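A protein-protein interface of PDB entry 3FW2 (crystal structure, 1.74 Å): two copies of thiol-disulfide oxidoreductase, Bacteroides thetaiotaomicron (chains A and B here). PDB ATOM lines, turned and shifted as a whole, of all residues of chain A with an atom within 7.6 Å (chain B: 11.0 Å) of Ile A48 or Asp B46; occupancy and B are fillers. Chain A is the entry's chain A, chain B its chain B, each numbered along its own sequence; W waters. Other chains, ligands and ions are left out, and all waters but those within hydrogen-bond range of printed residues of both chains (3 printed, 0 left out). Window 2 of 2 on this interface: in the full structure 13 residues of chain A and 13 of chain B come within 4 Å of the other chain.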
ATOM      1  N   TRP A  44     -14.799  -6.928  -2.409  1.00  0.00           N
ATOM      2  CA  TRP A  44     -14.785  -6.818  -3.854  1.00  0.00           C
ATOM      3  C   TRP A  44     -13.363  -6.645  -4.451  1.00  0.00           C
ATOM      4  O   TRP A  44     -13.198  -6.520  -5.710  1.00  0.00           O
ATOM      5  CB  TRP A  44     -15.726  -5.682  -4.320  1.00  0.00           C
ATOM      6  CG  TRP A  44     -15.490  -4.288  -3.769  1.00  0.00           C
ATOM      7  CD1 TRP A  44     -16.235  -3.661  -2.814  1.00  0.00           C
ATOM      8  CD2 TRP A  44     -14.489  -3.353  -4.173  1.00  0.00           C
ATOM      9  NE1 TRP A  44     -15.756  -2.398  -2.606  1.00  0.00           N
ATOM     10  CE2 TRP A  44     -14.688  -2.182  -3.432  1.00  0.00           C
ATOM     11  CE3 TRP A  44     -13.437  -3.385  -5.118  1.00  0.00           C
ATOM     12  CZ2 TRP A  44     -13.864  -1.040  -3.566  1.00  0.00           C
ATOM     13  CZ3 TRP A  44     -12.617  -2.229  -5.246  1.00  0.00           C
ATOM     14  CH2 TRP A  44     -12.833  -1.095  -4.470  1.00  0.00           C
ATOM     15  N   ASN A  45     -12.333  -6.637  -3.576  1.00  0.00           N
ATOM     16  CA  ASN A  45     -10.945  -6.673  -4.027  1.00  0.00           C
ATOM     17  C   ASN A  45     -10.167  -7.758  -3.308  1.00  0.00           C
ATOM     18  O   ASN A  45      -9.298  -7.478  -2.535  1.00  0.00           O
ATOM     19  CB  ASN A  45     -10.312  -5.301  -3.765  1.00  0.00           C
ATOM     20  CG  ASN A  45      -8.908  -5.203  -4.282  1.00  0.00           C
ATOM     21  OD1 ASN A  45      -8.654  -5.553  -5.406  1.00  0.00           O
ATOM     22  ND2 ASN A  45      -8.013  -4.727  -3.449  1.00  0.00           N
ATOM     23  N   ASP A  46     -10.487  -9.002  -3.602  1.00  0.00           N
ATOM     24  CA  ASP A  46      -9.822 -10.159  -2.954  1.00  0.00           C
ATOM     25  C   ASP A  46      -8.659 -10.503  -3.873  1.00  0.00           C
ATOM     26  O   ASP A  46      -8.632 -11.558  -4.534  1.00  0.00           O
ATOM     27  CB  ASP A  46     -10.842 -11.333  -2.827  1.00  0.00           C
ATOM     28  CG  ASP A  46     -10.316 -12.489  -1.970  1.00  0.00           C
ATOM     29  OD1 ASP A  46      -9.210 -12.359  -1.428  1.00  0.00           O
ATOM     30  OD2 ASP A  46     -11.017 -13.539  -1.887  1.00  0.00           O
ATOM     31  N   SER A  47      -7.683  -9.599  -3.907  1.00  0.00           N
ATOM     32  CA  SER A  47      -6.557  -9.666  -4.797  1.00  0.00           C
ATOM     33  C   SER A  47      -5.392 -10.411  -4.142  1.00  0.00           C
ATOM     34  O   SER A  47      -5.400 -10.701  -2.944  1.00  0.00           O
ATOM     35  CB  SER A  47      -6.098  -8.238  -5.085  1.00  0.00           C
ATOM     36  OG  SER A  47      -5.672  -7.653  -3.876  1.00  0.00           O
ATOM     37  N   ILE A  48      -4.348 -10.702  -4.913  1.00  0.00           N
ATOM     38  CA  ILE A  48      -3.122 -11.262  -4.314  1.00  0.00           C
ATOM     39  C   ILE A  48      -2.560 -10.339  -3.244  1.00  0.00           C
ATOM     40  O   ILE A  48      -2.127 -10.807  -2.193  1.00  0.00           O
ATOM     41  CB  ILE A  48      -2.018 -11.594  -5.429  1.00  0.00           C
ATOM     42  CG1 ILE A  48      -2.464 -12.747  -6.322  1.00  0.00           C
ATOM     43  CG2 ILE A  48      -0.736 -11.905  -4.726  1.00  0.00           C
ATOM     44  CD1 ILE A  48      -1.860 -12.662  -7.784  1.00  0.00           C
ATOM     45  N   SER A  49      -2.551  -9.009  -3.489  1.00  0.00           N
ATOM     46  CA  SER A  49      -2.007  -8.080  -2.487  1.00  0.00           C
ATOM     47  C   SER A  49      -2.863  -8.107  -1.241  1.00  0.00           C
ATOM     48  O   SER A  49      -2.349  -8.079  -0.131  1.00  0.00           O
ATOM     49  CB  SER A  49      -1.966  -6.637  -3.015  1.00  0.00           C
ATOM     50  OG  SER A  49      -1.026  -6.559  -4.068  1.00  0.00           O
ATOM     51  N   GLN A  50      -4.162  -8.146  -1.410  1.00  0.00           N
ATOM     52  CA  GLN A  50      -5.024  -8.214  -0.213  1.00  0.00           C
ATOM     53  C   GLN A  50      -4.806  -9.522   0.567  1.00  0.00           C
ATOM     54  O   GLN A  50      -4.757  -9.510   1.808  1.00  0.00           O
ATOM     55  CB  GLN A  50      -6.519  -8.067  -0.529  1.00  0.00           C
ATOM     56  CG  GLN A  50      -7.381  -7.975   0.817  1.00  0.00           C
ATOM     57  CD  GLN A  50      -7.027  -6.767   1.598  1.00  0.00           C
ATOM     58  OE1 GLN A  50      -7.104  -5.655   1.047  1.00  0.00           O
ATOM     59  NE2 GLN A  50      -6.545  -6.922   2.918  1.00  0.00           N
ATOM     60  N   LYS A  51      -4.667 -10.630  -0.133  1.00  0.00           N
ATOM     61  CA  LYS A  51      -4.365 -11.866   0.529  1.00  0.00           C
ATOM     62  C   LYS A  51      -3.027 -11.794   1.306  1.00  0.00           C
ATOM     63  O   LYS A  51      -2.897 -12.302   2.426  1.00  0.00           O
ATOM     64  CB  LYS A  51      -4.419 -13.021  -0.445  1.00  0.00           C
ATOM     65  CG  LYS A  51      -5.826 -13.386  -0.958  1.00  0.00           C
ATOM     66  CD  LYS A  51      -5.771 -14.553  -1.912  1.00  0.00           C
ATOM     67  CE  LYS A  51      -7.162 -15.020  -2.338  1.00  0.00           C
ATOM     68  NZ  LYS A  51      -7.734 -13.962  -3.191  1.00  0.00           N
ATOM     69  N   GLN A  52      -2.024 -11.166   0.706  1.00  0.00           N
ATOM     70  CA  GLN A  52      -0.741 -11.003   1.386  1.00  0.00           C
ATOM     71  C   GLN A  52      -0.904 -10.149   2.642  1.00  0.00           C
ATOM     72  O   GLN A  52      -0.370 -10.460   3.715  1.00  0.00           O
ATOM     73  CB  GLN A  52       0.235 -10.287   0.449  1.00  0.00           C
ATOM     74  CG  GLN A  52       1.621 -10.090   1.037  1.00  0.00           C
ATOM     75  CD  GLN A  52       2.316 -11.346   1.462  1.00  0.00           C
ATOM     76  OE1 GLN A  52       2.241 -12.365   0.782  1.00  0.00           O
ATOM     77  NE2 GLN A  52       3.045 -11.274   2.595  1.00  0.00           N
ATOM     78  N   SER A  53      -1.584  -9.002   2.523  1.00  0.00           N
ATOM     79  CA  SER A  53      -1.829  -8.176   3.680  1.00  0.00           C
ATOM     80  C   SER A  53      -2.534  -8.949   4.793  1.00  0.00           C
ATOM     81  O   SER A  53      -2.162  -8.874   5.939  1.00  0.00           O
ATOM     82  CB  SER A  53      -2.696  -6.977   3.296  1.00  0.00           C
ATOM     83  OG  SER A  53      -1.952  -6.104   2.483  1.00  0.00           O
ATOM     84  N   ASN A  54      -3.547  -9.705   4.419  1.00  0.00           N
ATOM     85  CA  ASN A  54      -4.297 -10.488   5.373  1.00  0.00           C
ATOM     86  C   ASN A  54      -3.393 -11.490   6.059  1.00  0.00           C
ATOM     87  O   ASN A  54      -3.500 -11.679   7.269  1.00  0.00           O
ATOM     88  CB  ASN A  54      -5.434 -11.218   4.658  1.00  0.00           C
ATOM     89  CG  ASN A  54      -6.594 -10.307   4.313  1.00  0.00           C
ATOM     90  OD1 ASN A  54      -6.663  -9.129   4.758  1.00  0.00           O
ATOM     91  ND2 ASN A  54      -7.533 -10.836   3.549  1.00  0.00           N
ATOM     92  N   SER A  55      -2.518 -12.142   5.297  1.00  0.00           N
ATOM     93  CA  SER A  55      -1.590 -13.103   5.928  1.00  0.00           C
ATOM     94  C   SER A  55      -0.760 -12.405   6.990  1.00  0.00           C
ATOM     95  O   SER A  55      -0.537 -12.910   8.098  1.00  0.00           O
ATOM     96  CB  SER A  55      -0.651 -13.752   4.870  1.00  0.00           C
ATOM     97  OG  SER A  55      -1.415 -14.499   3.908  1.00  0.00           O
ATOM     98  N   PRO A 118      -5.149  -2.969  -0.823  1.00  0.00           N
ATOM     99  CA  PRO A 118      -5.089  -2.668   0.593  1.00  0.00           C
ATOM    100  C   PRO A 118      -4.281  -1.453   0.933  1.00  0.00           C
ATOM    101  O   PRO A 118      -3.352  -1.041   0.177  1.00  0.00           O
ATOM    102  CB  PRO A 118      -4.403  -3.901   1.191  1.00  0.00           C
ATOM    103  CG  PRO A 118      -3.652  -4.463   0.055  1.00  0.00           C
ATOM    104  CD  PRO A 118      -4.507  -4.253  -1.127  1.00  0.00           C
ATOM    105  N   PHE B  40     -14.398   1.749 -15.818  1.00  0.00           N
ATOM    106  CA  PHE B  40     -13.469   2.082 -14.740  1.00  0.00           C
ATOM    107  C   PHE B  40     -12.908   0.813 -14.111  1.00  0.00           C
ATOM    108  O   PHE B  40     -13.608  -0.173 -13.914  1.00  0.00           O
ATOM    109  CB  PHE B  40     -14.187   2.851 -13.665  1.00  0.00           C
ATOM    110  CG  PHE B  40     -14.688   4.199 -14.113  1.00  0.00           C
ATOM    111  CD1 PHE B  40     -13.901   5.332 -13.937  1.00  0.00           C
ATOM    112  CD2 PHE B  40     -15.976   4.332 -14.607  1.00  0.00           C
ATOM    113  CE1 PHE B  40     -14.360   6.567 -14.331  1.00  0.00           C
ATOM    114  CE2 PHE B  40     -16.443   5.567 -15.011  1.00  0.00           C
ATOM    115  CZ  PHE B  40     -15.638   6.685 -14.866  1.00  0.00           C
ATOM    116  N   TRP B  41     -11.589   0.813 -13.874  1.00  0.00           N
ATOM    117  CA  TRP B  41     -10.916  -0.361 -13.433  1.00  0.00           C
ATOM    118  C   TRP B  41      -9.607   0.067 -12.757  1.00  0.00           C
ATOM    119  O   TRP B  41      -9.283   1.263 -12.759  1.00  0.00           O
ATOM    120  CB  TRP B  41     -10.652  -1.284 -14.641  1.00  0.00           C
ATOM    121  CG  TRP B  41      -9.681  -0.715 -15.635  1.00  0.00           C
ATOM    122  CD1 TRP B  41      -9.860   0.356 -16.440  1.00  0.00           C
ATOM    123  CD2 TRP B  41      -8.330  -1.129 -15.817  1.00  0.00           C
ATOM    124  NE1 TRP B  41      -8.738   0.575 -17.212  1.00  0.00           N
ATOM    125  CE2 TRP B  41      -7.788  -0.346 -16.854  1.00  0.00           C
ATOM    126  CE3 TRP B  41      -7.568  -2.165 -15.296  1.00  0.00           C
ATOM    127  CZ2 TRP B  41      -6.471  -0.493 -17.310  1.00  0.00           C
ATOM    128  CZ3 TRP B  41      -6.243  -2.361 -15.798  1.00  0.00           C
ATOM    129  CH2 TRP B  41      -5.716  -1.512 -16.778  1.00  0.00           C
ATOM    130  N   ALA B  42      -8.852  -0.929 -12.274  1.00  0.00           N
ATOM    131  CA  ALA B  42      -7.438  -0.713 -11.887  1.00  0.00           C
ATOM    132  C   ALA B  42      -6.685  -2.018 -11.963  1.00  0.00           C
ATOM    133  O   ALA B  42      -7.233  -3.092 -11.696  1.00  0.00           O
ATOM    134  CB  ALA B  42      -7.321  -0.124 -10.498  1.00  0.00           C
ATOM    135  N   SER B  43      -5.402  -1.946 -12.306  1.00  0.00           N
ATOM    136  CA  SER B  43      -4.647  -3.191 -12.492  1.00  0.00           C
ATOM    137  C   SER B  43      -4.490  -3.999 -11.260  1.00  0.00           C
ATOM    138  O   SER B  43      -4.353  -5.252 -11.319  1.00  0.00           O
ATOM    139  CB  SER B  43      -3.230  -2.894 -13.064  1.00  0.00           C
ATOM    140  OG  SER B  43      -2.432  -2.263 -12.078  1.00  0.00           O
ATOM    141  N   TRP B  44      -4.504  -3.320 -10.145  1.00  0.00           N
ATOM    142  CA  TRP B  44      -4.375  -3.972  -8.858  1.00  0.00           C
ATOM    143  C   TRP B  44      -5.632  -4.705  -8.387  1.00  0.00           C
ATOM    144  O   TRP B  44      -5.566  -5.453  -7.417  1.00  0.00           O
ATOM    145  CB  TRP B  44      -3.919  -2.997  -7.780  1.00  0.00           C
ATOM    146  CG  TRP B  44      -4.682  -1.712  -7.592  1.00  0.00           C
ATOM    147  CD1 TRP B  44      -4.282  -0.489  -7.958  1.00  0.00           C
ATOM    148  CD2 TRP B  44      -5.978  -1.535  -6.977  1.00  0.00           C
ATOM    149  NE1 TRP B  44      -5.198   0.454  -7.626  1.00  0.00           N
ATOM    150  CE2 TRP B  44      -6.255  -0.162  -7.007  1.00  0.00           C
ATOM    151  CE3 TRP B  44      -6.904  -2.399  -6.379  1.00  0.00           C
ATOM    152  CZ2 TRP B  44      -7.438   0.388  -6.522  1.00  0.00           C
ATOM    153  CZ3 TRP B  44      -8.097  -1.835  -5.890  1.00  0.00           C
ATOM    154  CH2 TRP B  44      -8.347  -0.490  -5.940  1.00  0.00           C
ATOM    155  N   ASN B  45      -6.757  -4.471  -9.058  1.00  0.00           N
ATOM    156  CA  ASN B  45      -8.029  -5.087  -8.670  1.00  0.00           C
ATOM    157  C   ASN B  45      -8.187  -6.394  -9.427  1.00  0.00           C
ATOM    158  O   ASN B  45      -9.061  -6.514 -10.268  1.00  0.00           O
ATOM    159  CB  ASN B  45      -9.162  -4.090  -8.994  1.00  0.00           C
ATOM    160  CG  ASN B  45     -10.557  -4.604  -8.647  1.00  0.00           C
ATOM    161  OD1 ASN B  45     -11.478  -4.381  -9.422  1.00  0.00           O
ATOM    162  ND2 ASN B  45     -10.708  -5.223  -7.490  1.00  0.00           N
ATOM    163  N   ASP B  46      -7.338  -7.361  -9.034  1.00  0.00           N
ATOM    164  CA  ASP B  46      -7.338  -8.721  -9.625  1.00  0.00           C
ATOM    165  C   ASP B  46      -8.511  -9.611  -9.160  1.00  0.00           C
ATOM    166  O   ASP B  46      -8.309 -10.745  -8.733  1.00  0.00           O
ATOM    167  CB  ASP B  46      -5.953  -9.487  -9.589  1.00  0.00           C
ATOM    168  CG  ASP B  46      -5.035  -9.232  -8.330  1.00  0.00           C
ATOM    169  OD1 ASP B  46      -4.653 -10.247  -7.649  1.00  0.00           O
ATOM    170  OD2 ASP B  46      -4.510  -8.105  -8.124  1.00  0.00           O
ATOM    171  N   SER B  47      -9.741  -9.103  -9.287  1.00  0.00           N
ATOM    172  CA  SER B  47     -10.930  -9.826  -8.835  1.00  0.00           C
ATOM    173  C   SER B  47     -11.677 -10.609  -9.872  1.00  0.00           C
ATOM    174  O   SER B  47     -11.513 -10.431 -11.091  1.00  0.00           O
ATOM    175  CB  SER B  47     -11.933  -8.783  -8.311  1.00  0.00           C
ATOM    176  OG  SER B  47     -12.493  -7.990  -9.380  1.00  0.00           O
ATOM    177  N   ILE B  48     -12.580 -11.466  -9.411  1.00  0.00           N
ATOM    178  CA  ILE B  48     -13.423 -12.199 -10.366  1.00  0.00           C
ATOM    179  C   ILE B  48     -14.278 -11.286 -11.203  1.00  0.00           C
ATOM    180  O   ILE B  48     -14.423 -11.502 -12.400  1.00  0.00           O
ATOM    181  CB  ILE B  48     -14.291 -13.319  -9.711  1.00  0.00           C
ATOM    182  CG1 ILE B  48     -13.414 -14.521  -9.378  1.00  0.00           C
ATOM    183  CG2 ILE B  48     -15.323 -13.822 -10.744  1.00  0.00           C
ATOM    184  CD1 ILE B  48     -13.013 -15.372 -10.672  1.00  0.00           C
ATOM    185  N   SER B  49     -14.834 -10.235 -10.587  1.00  0.00           N
ATOM    186  CA  SER B  49     -15.620  -9.269 -11.357  1.00  0.00           C
ATOM    187  C   SER B  49     -14.772  -8.591 -12.432  1.00  0.00           C
ATOM    188  O   SER B  49     -15.243  -8.408 -13.561  1.00  0.00           O
ATOM    189  CB  SER B  49     -16.300  -8.208 -10.492  1.00  0.00           C
ATOM    190  OG  SER B  49     -17.276  -7.504 -11.270  1.00  0.00           O
ATOM    191  N   GLN B  50     -13.550  -8.215 -12.097  1.00  0.00           N
ATOM    192  CA  GLN B  50     -12.668  -7.583 -13.075  1.00  0.00           C
ATOM    193  C   GLN B  50     -12.321  -8.544 -14.248  1.00  0.00           C
ATOM    194  O   GLN B  50     -12.320  -8.149 -15.372  1.00  0.00           O
ATOM    195  CB  GLN B  50     -11.371  -7.100 -12.396  1.00  0.00           C
ATOM    196  CG  GLN B  50     -10.312  -6.593 -13.373  1.00  0.00           C
ATOM    197  CD  GLN B  50     -10.716  -5.344 -14.118  1.00  0.00           C
ATOM    198  OE1 GLN B  50     -11.796  -4.819 -13.922  1.00  0.00           O
ATOM    199  NE2 GLN B  50      -9.833  -4.863 -15.023  1.00  0.00           N
ATOM    200  N   LYS B  51     -12.054  -9.810 -13.968  1.00  0.00           N
ATOM    201  CA  LYS B  51     -11.759 -10.772 -15.031  1.00  0.00           C
ATOM    202  C   LYS B  51     -12.959 -10.960 -15.976  1.00  0.00           C
ATOM    203  O   LYS B  51     -12.832 -10.996 -17.207  1.00  0.00           O
ATOM    204  CB  LYS B  51     -11.305 -12.068 -14.361  1.00  0.00           C
ATOM    205  CG  LYS B  51      -9.964 -11.854 -13.620  1.00  0.00           C
ATOM    206  CD  LYS B  51      -9.307 -13.114 -13.053  1.00  0.00           C
ATOM    207  CE  LYS B  51      -8.199 -12.731 -12.033  1.00  0.00           C
ATOM    208  NZ  LYS B  51      -7.080 -13.707 -11.912  1.00  0.00           N
ATOM    209  N   GLN B  52     -14.155 -11.036 -15.381  1.00  0.00           N
ATOM    210  CA  GLN B  52     -15.364 -11.237 -16.146  1.00  0.00           C
ATOM    211  C   GLN B  52     -15.692  -9.989 -16.918  1.00  0.00           C
ATOM    212  O   GLN B  52     -16.107 -10.037 -18.081  1.00  0.00           O
ATOM    213  CB  GLN B  52     -16.521 -11.619 -15.218  1.00  0.00           C
ATOM    214  CG  GLN B  52     -17.834 -11.761 -15.930  1.00  0.00           C
ATOM    215  CD  GLN B  52     -17.813 -12.834 -16.998  1.00  0.00           C
ATOM    216  OE1 GLN B  52     -17.043 -13.801 -16.917  1.00  0.00           O
ATOM    217  NE2 GLN B  52     -18.669 -12.678 -18.006  1.00  0.00           N
ATOM    218  N   SER B  53     -15.488  -8.838 -16.271  1.00  0.00           N
ATOM    219  CA  SER B  53     -15.723  -7.588 -16.931  1.00  0.00           C
ATOM    220  C   SER B  53     -14.818  -7.452 -18.134  1.00  0.00           C
ATOM    221  O   SER B  53     -15.260  -7.032 -19.182  1.00  0.00           O
ATOM    222  CB  SER B  53     -15.498  -6.408 -15.949  1.00  0.00           C
ATOM    223  OG  SER B  53     -15.425  -5.190 -16.635  1.00  0.00           O
ATOM    224  N   ASN B  54     -13.537  -7.783 -17.983  1.00  0.00           N
ATOM    225  CA  ASN B  54     -12.624  -7.631 -19.082  1.00  0.00           C
ATOM    226  C   ASN B  54     -13.026  -8.513 -20.253  1.00  0.00           C
ATOM    227  O   ASN B  54     -12.986  -8.073 -21.375  1.00  0.00           O
ATOM    228  CB  ASN B  54     -11.200  -7.959 -18.684  1.00  0.00           C
ATOM    229  CG  ASN B  54     -10.516  -6.834 -17.933  1.00  0.00           C
ATOM    230  OD1 ASN B  54     -10.978  -5.655 -17.886  1.00  0.00           O
ATOM    231  ND2 ASN B  54      -9.388  -7.201 -17.308  1.00  0.00           N
ATOM    232  N   SER B  76      -8.499   4.076 -15.866  1.00  0.00           N
ATOM    233  CA  SER B  76      -7.911   3.385 -14.751  1.00  0.00           C
ATOM    234  C   SER B  76      -7.686   4.273 -13.528  1.00  0.00           C
ATOM    235  O   SER B  76      -7.351   5.449 -13.638  1.00  0.00           O
ATOM    236  CB  SER B  76      -6.596   2.713 -15.109  1.00  0.00           C
ATOM    237  OG  SER B  76      -5.977   2.175 -13.935  1.00  0.00           O
ATOM    238  N   ASP B  78      -5.466   3.300 -11.341  1.00  0.00           N
ATOM    239  CA  ASP B  78      -4.062   3.032 -10.988  1.00  0.00           C
ATOM    240  C   ASP B  78      -3.289   4.257 -10.571  1.00  0.00           C
ATOM    241  O   ASP B  78      -3.593   5.365 -10.999  1.00  0.00           O
ATOM    242  CB  ASP B  78      -3.327   2.394 -12.187  1.00  0.00           C
ATOM    243  CG  ASP B  78      -3.575   0.886 -12.287  1.00  0.00           C
ATOM    244  OD1 ASP B  78      -3.134   0.170 -11.361  1.00  0.00           O
ATOM    245  OD2 ASP B  78      -4.169   0.467 -13.285  1.00  0.00           O
ATOM    246  N   GLN B  83       2.505  -0.765 -13.934  1.00  0.00           N
ATOM    247  CA  GLN B  83       1.468  -1.787 -13.621  1.00  0.00           C
ATOM    248  C   GLN B  83       0.263  -1.638 -14.527  1.00  0.00           C
ATOM    249  O   GLN B  83      -0.304  -2.613 -15.042  1.00  0.00           O
ATOM    250  CB  GLN B  83       1.050  -1.707 -12.146  1.00  0.00           C
ATOM    251  CG  GLN B  83       2.111  -2.138 -11.205  1.00  0.00           C
ATOM    252  CD  GLN B  83       2.305  -3.595 -11.209  1.00  0.00           C
ATOM    253  OE1 GLN B  83       1.339  -4.369 -11.332  1.00  0.00           O
ATOM    254  NE2 GLN B  83       3.552  -4.014 -11.075  1.00  0.00           N
ATOM    255  N   ALA B  87      -0.866  -4.416 -17.388  1.00  0.00           N
ATOM    256  CA  ALA B  87      -2.232  -4.980 -17.443  1.00  0.00           C
ATOM    257  C   ALA B  87      -2.882  -4.793 -18.795  1.00  0.00           C
ATOM    258  O   ALA B  87      -3.555  -5.726 -19.269  1.00  0.00           O
ATOM    259  CB  ALA B  87      -3.132  -4.455 -16.353  1.00  0.00           C
ATOM    260  N   ARG B  90      -1.261  -7.469 -20.991  1.00  0.00           N
ATOM    261  CA  ARG B  90      -1.634  -8.811 -20.582  1.00  0.00           C
ATOM    262  C   ARG B  90      -3.107  -9.138 -20.908  1.00  0.00           C
ATOM    263  O   ARG B  90      -3.430 -10.294 -21.308  1.00  0.00           O
ATOM    264  CB  ARG B  90      -1.405  -8.909 -19.076  1.00  0.00           C
ATOM    265  CG  ARG B  90      -1.906 -10.129 -18.353  1.00  0.00           C
ATOM    266  CD  ARG B  90      -1.474 -10.026 -16.851  1.00  0.00           C
ATOM    267  NE  ARG B  90      -0.174  -9.364 -16.618  1.00  0.00           N
ATOM    268  CZ  ARG B  90       0.033  -8.248 -15.882  1.00  0.00           C
ATOM    269  NH1 ARG B  90       1.274  -7.777 -15.731  1.00  0.00           N
ATOM    270  NH2 ARG B  90      -0.955  -7.605 -15.273  1.00  0.00           N
ATOM    271  N   ASP B  91      -3.988  -8.148 -20.720  1.00  0.00           N
ATOM    272  CA  ASP B  91      -5.441  -8.369 -20.829  1.00  0.00           C
ATOM    273  C   ASP B  91      -5.991  -7.818 -22.143  1.00  0.00           C
ATOM    274  O   ASP B  91      -7.216  -7.725 -22.328  1.00  0.00           O
ATOM    275  CB  ASP B  91      -6.148  -7.735 -19.616  1.00  0.00           C
ATOM    276  CG  ASP B  91      -5.763  -8.374 -18.282  1.00  0.00           C
ATOM    277  OD1 ASP B  91      -5.440  -9.556 -18.257  1.00  0.00           O
ATOM    278  OD2 ASP B  91      -5.773  -7.676 -17.254  1.00  0.00           O
ATOM    279  N   ILE B 117     -14.949  -0.824  -8.049  1.00  0.00           N
ATOM    280  CA  ILE B 117     -14.520  -1.166  -9.371  1.00  0.00           C
ATOM    281  C   ILE B 117     -14.591  -2.715  -9.502  1.00  0.00           C
ATOM    282  O   ILE B 117     -14.495  -3.455  -8.512  1.00  0.00           O
ATOM    283  CB  ILE B 117     -13.119  -0.666  -9.746  1.00  0.00           C
ATOM    284  CG1 ILE B 117     -12.100  -0.902  -8.631  1.00  0.00           C
ATOM    285  CG2 ILE B 117     -13.184   0.816 -10.097  1.00  0.00           C
ATOM    286  CD1 ILE B 117     -10.636  -0.599  -9.050  1.00  0.00           C
ATOM    287  N   PRO B 118     -14.738  -3.185 -10.750  1.00  0.00           N
ATOM    288  CA  PRO B 118     -15.002  -2.474 -11.959  1.00  0.00           C
ATOM    289  C   PRO B 118     -16.403  -1.783 -11.970  1.00  0.00           C
ATOM    290  O   PRO B 118     -17.311  -2.130 -11.194  1.00  0.00           O
ATOM    291  CB  PRO B 118     -14.984  -3.578 -13.050  1.00  0.00           C
ATOM    292  CG  PRO B 118     -15.302  -4.745 -12.374  1.00  0.00           C
ATOM    293  CD  PRO B 118     -14.732  -4.647 -10.973  1.00  0.00           C
HETATM  294  O   HOH W   1      -2.719  -7.781  -6.176  1.00  0.00           O
HETATM  295  O   HOH W   2     -14.176  -6.118  -8.014  1.00  0.00           O
HETATM  296  O   HOH W   3      -5.060  -5.080  -4.535  1.00  0.00           O
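O of Trp A44 is in hydrogen-bond range of ND2 of Asn B45 (3.3 Å). The side-chain amide nitrogen of Asn B45 is in hydrogen-bond range of the side-chain amide oxygen of Asn A45 (2.9 Å). The side-chain carboxylate (OD1) of Asp B46 lies within hydrogen-bond range of the backbone NH (N) of Ile A48 (2.8 Å).
The side-chain hydroxyl (OG) of Ser A47 lies close to the backbone NH (N) of Ser A49, 3.4 Å away. OG of Ser A47 is in hydrogen-bond range of N of Gln A50 (2.9 Å). OD1 of Asn B45 lies close to O of Ile B117, 3.3 Å away. The backbone NH (N) of Ser B49 sits close to the side-chain hydroxyl (OG) of Ser B47. The backbone NH (N) of Gln B50 lies within hydrogen-bond range of the side-chain hydroxyl (OG) of Ser B47, 2.9 Å away.
Among the printed residues, pairs that only touch across the chains: Trp A44 with Ser B47, Trp A44 with Ile B117, Asn A45 with Trp B44, Ser A47 with Trp B44 and Ser A47 with Asp B46.
Printed residues of chain B within 4 Å of Ile A48: Asp B46 (2.8 Å). No residue of chain B comes within 4 Å of Lys A51. Printed residues of chain A within 4 Å of Asn B45: Trp A44 (3.3 Å) and Asn A45 (2.9 Å). Printed residues of chain A within 4 Å of Asp B46: Ser A47 and Ile A48. Printed residues of chain A within 4 Å of Ser B47: Trp A44 (3.7 Å). Gln B83 touches none of the printed residues of chain A. Of the printed residues of chain A, Ile B117 touches Trp A44. The nearest printed residue of chain A that does not touch Asp B46 is Asn A45 (4.3 Å).
Hydrophobic or aromatic side chains of chain B within 4 Å of the printed part of chain A: Trp B44 and Ile B117. Hydrophobic or aromatic side chains of chain A within 4 Å of the printed part of chain B: Trp A44 and Ile A48. Among the printed residues, no Asp or Glu carboxylate lies within 4 Å of a Lys or Arg side-chain nitrogen of the other chain.
Trp A44 touches Ser B47, and with the chains exchanged Ser A47 touches Trp B44. Asn B45 touches its own counterpart, Asn A45. Ser A47 touches Asp B46, but with the chains exchanged Asp A46 does not touch Ser B47 (4.9 Å). Ile A48 touches Asp B46, but with the chains exchanged Asp A46 does not touch Ile B48 (6.3 Å).
Water W2 lies within hydrogen-bond range of O of Trp A44 (2.5 Å), O of Ile B117 (2.7 Å) and OG of Ser B47 (2.9 Å). Water W1 lies within hydrogen-bond range of the side-chain carboxylate of Asp B46 (2.7 Å) and the backbone NH of Ser A49 (3.0 Å). Water W3 lies within hydrogen-bond range of the side-chain hydroxyl (OG) of Ser A47 (2.7 Å), the backbone carbonyl oxygen (O) of Trp B44 (2.9 Å) and the side-chain amide nitrogen (ND2) of Asn A45 (3.2 Å).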
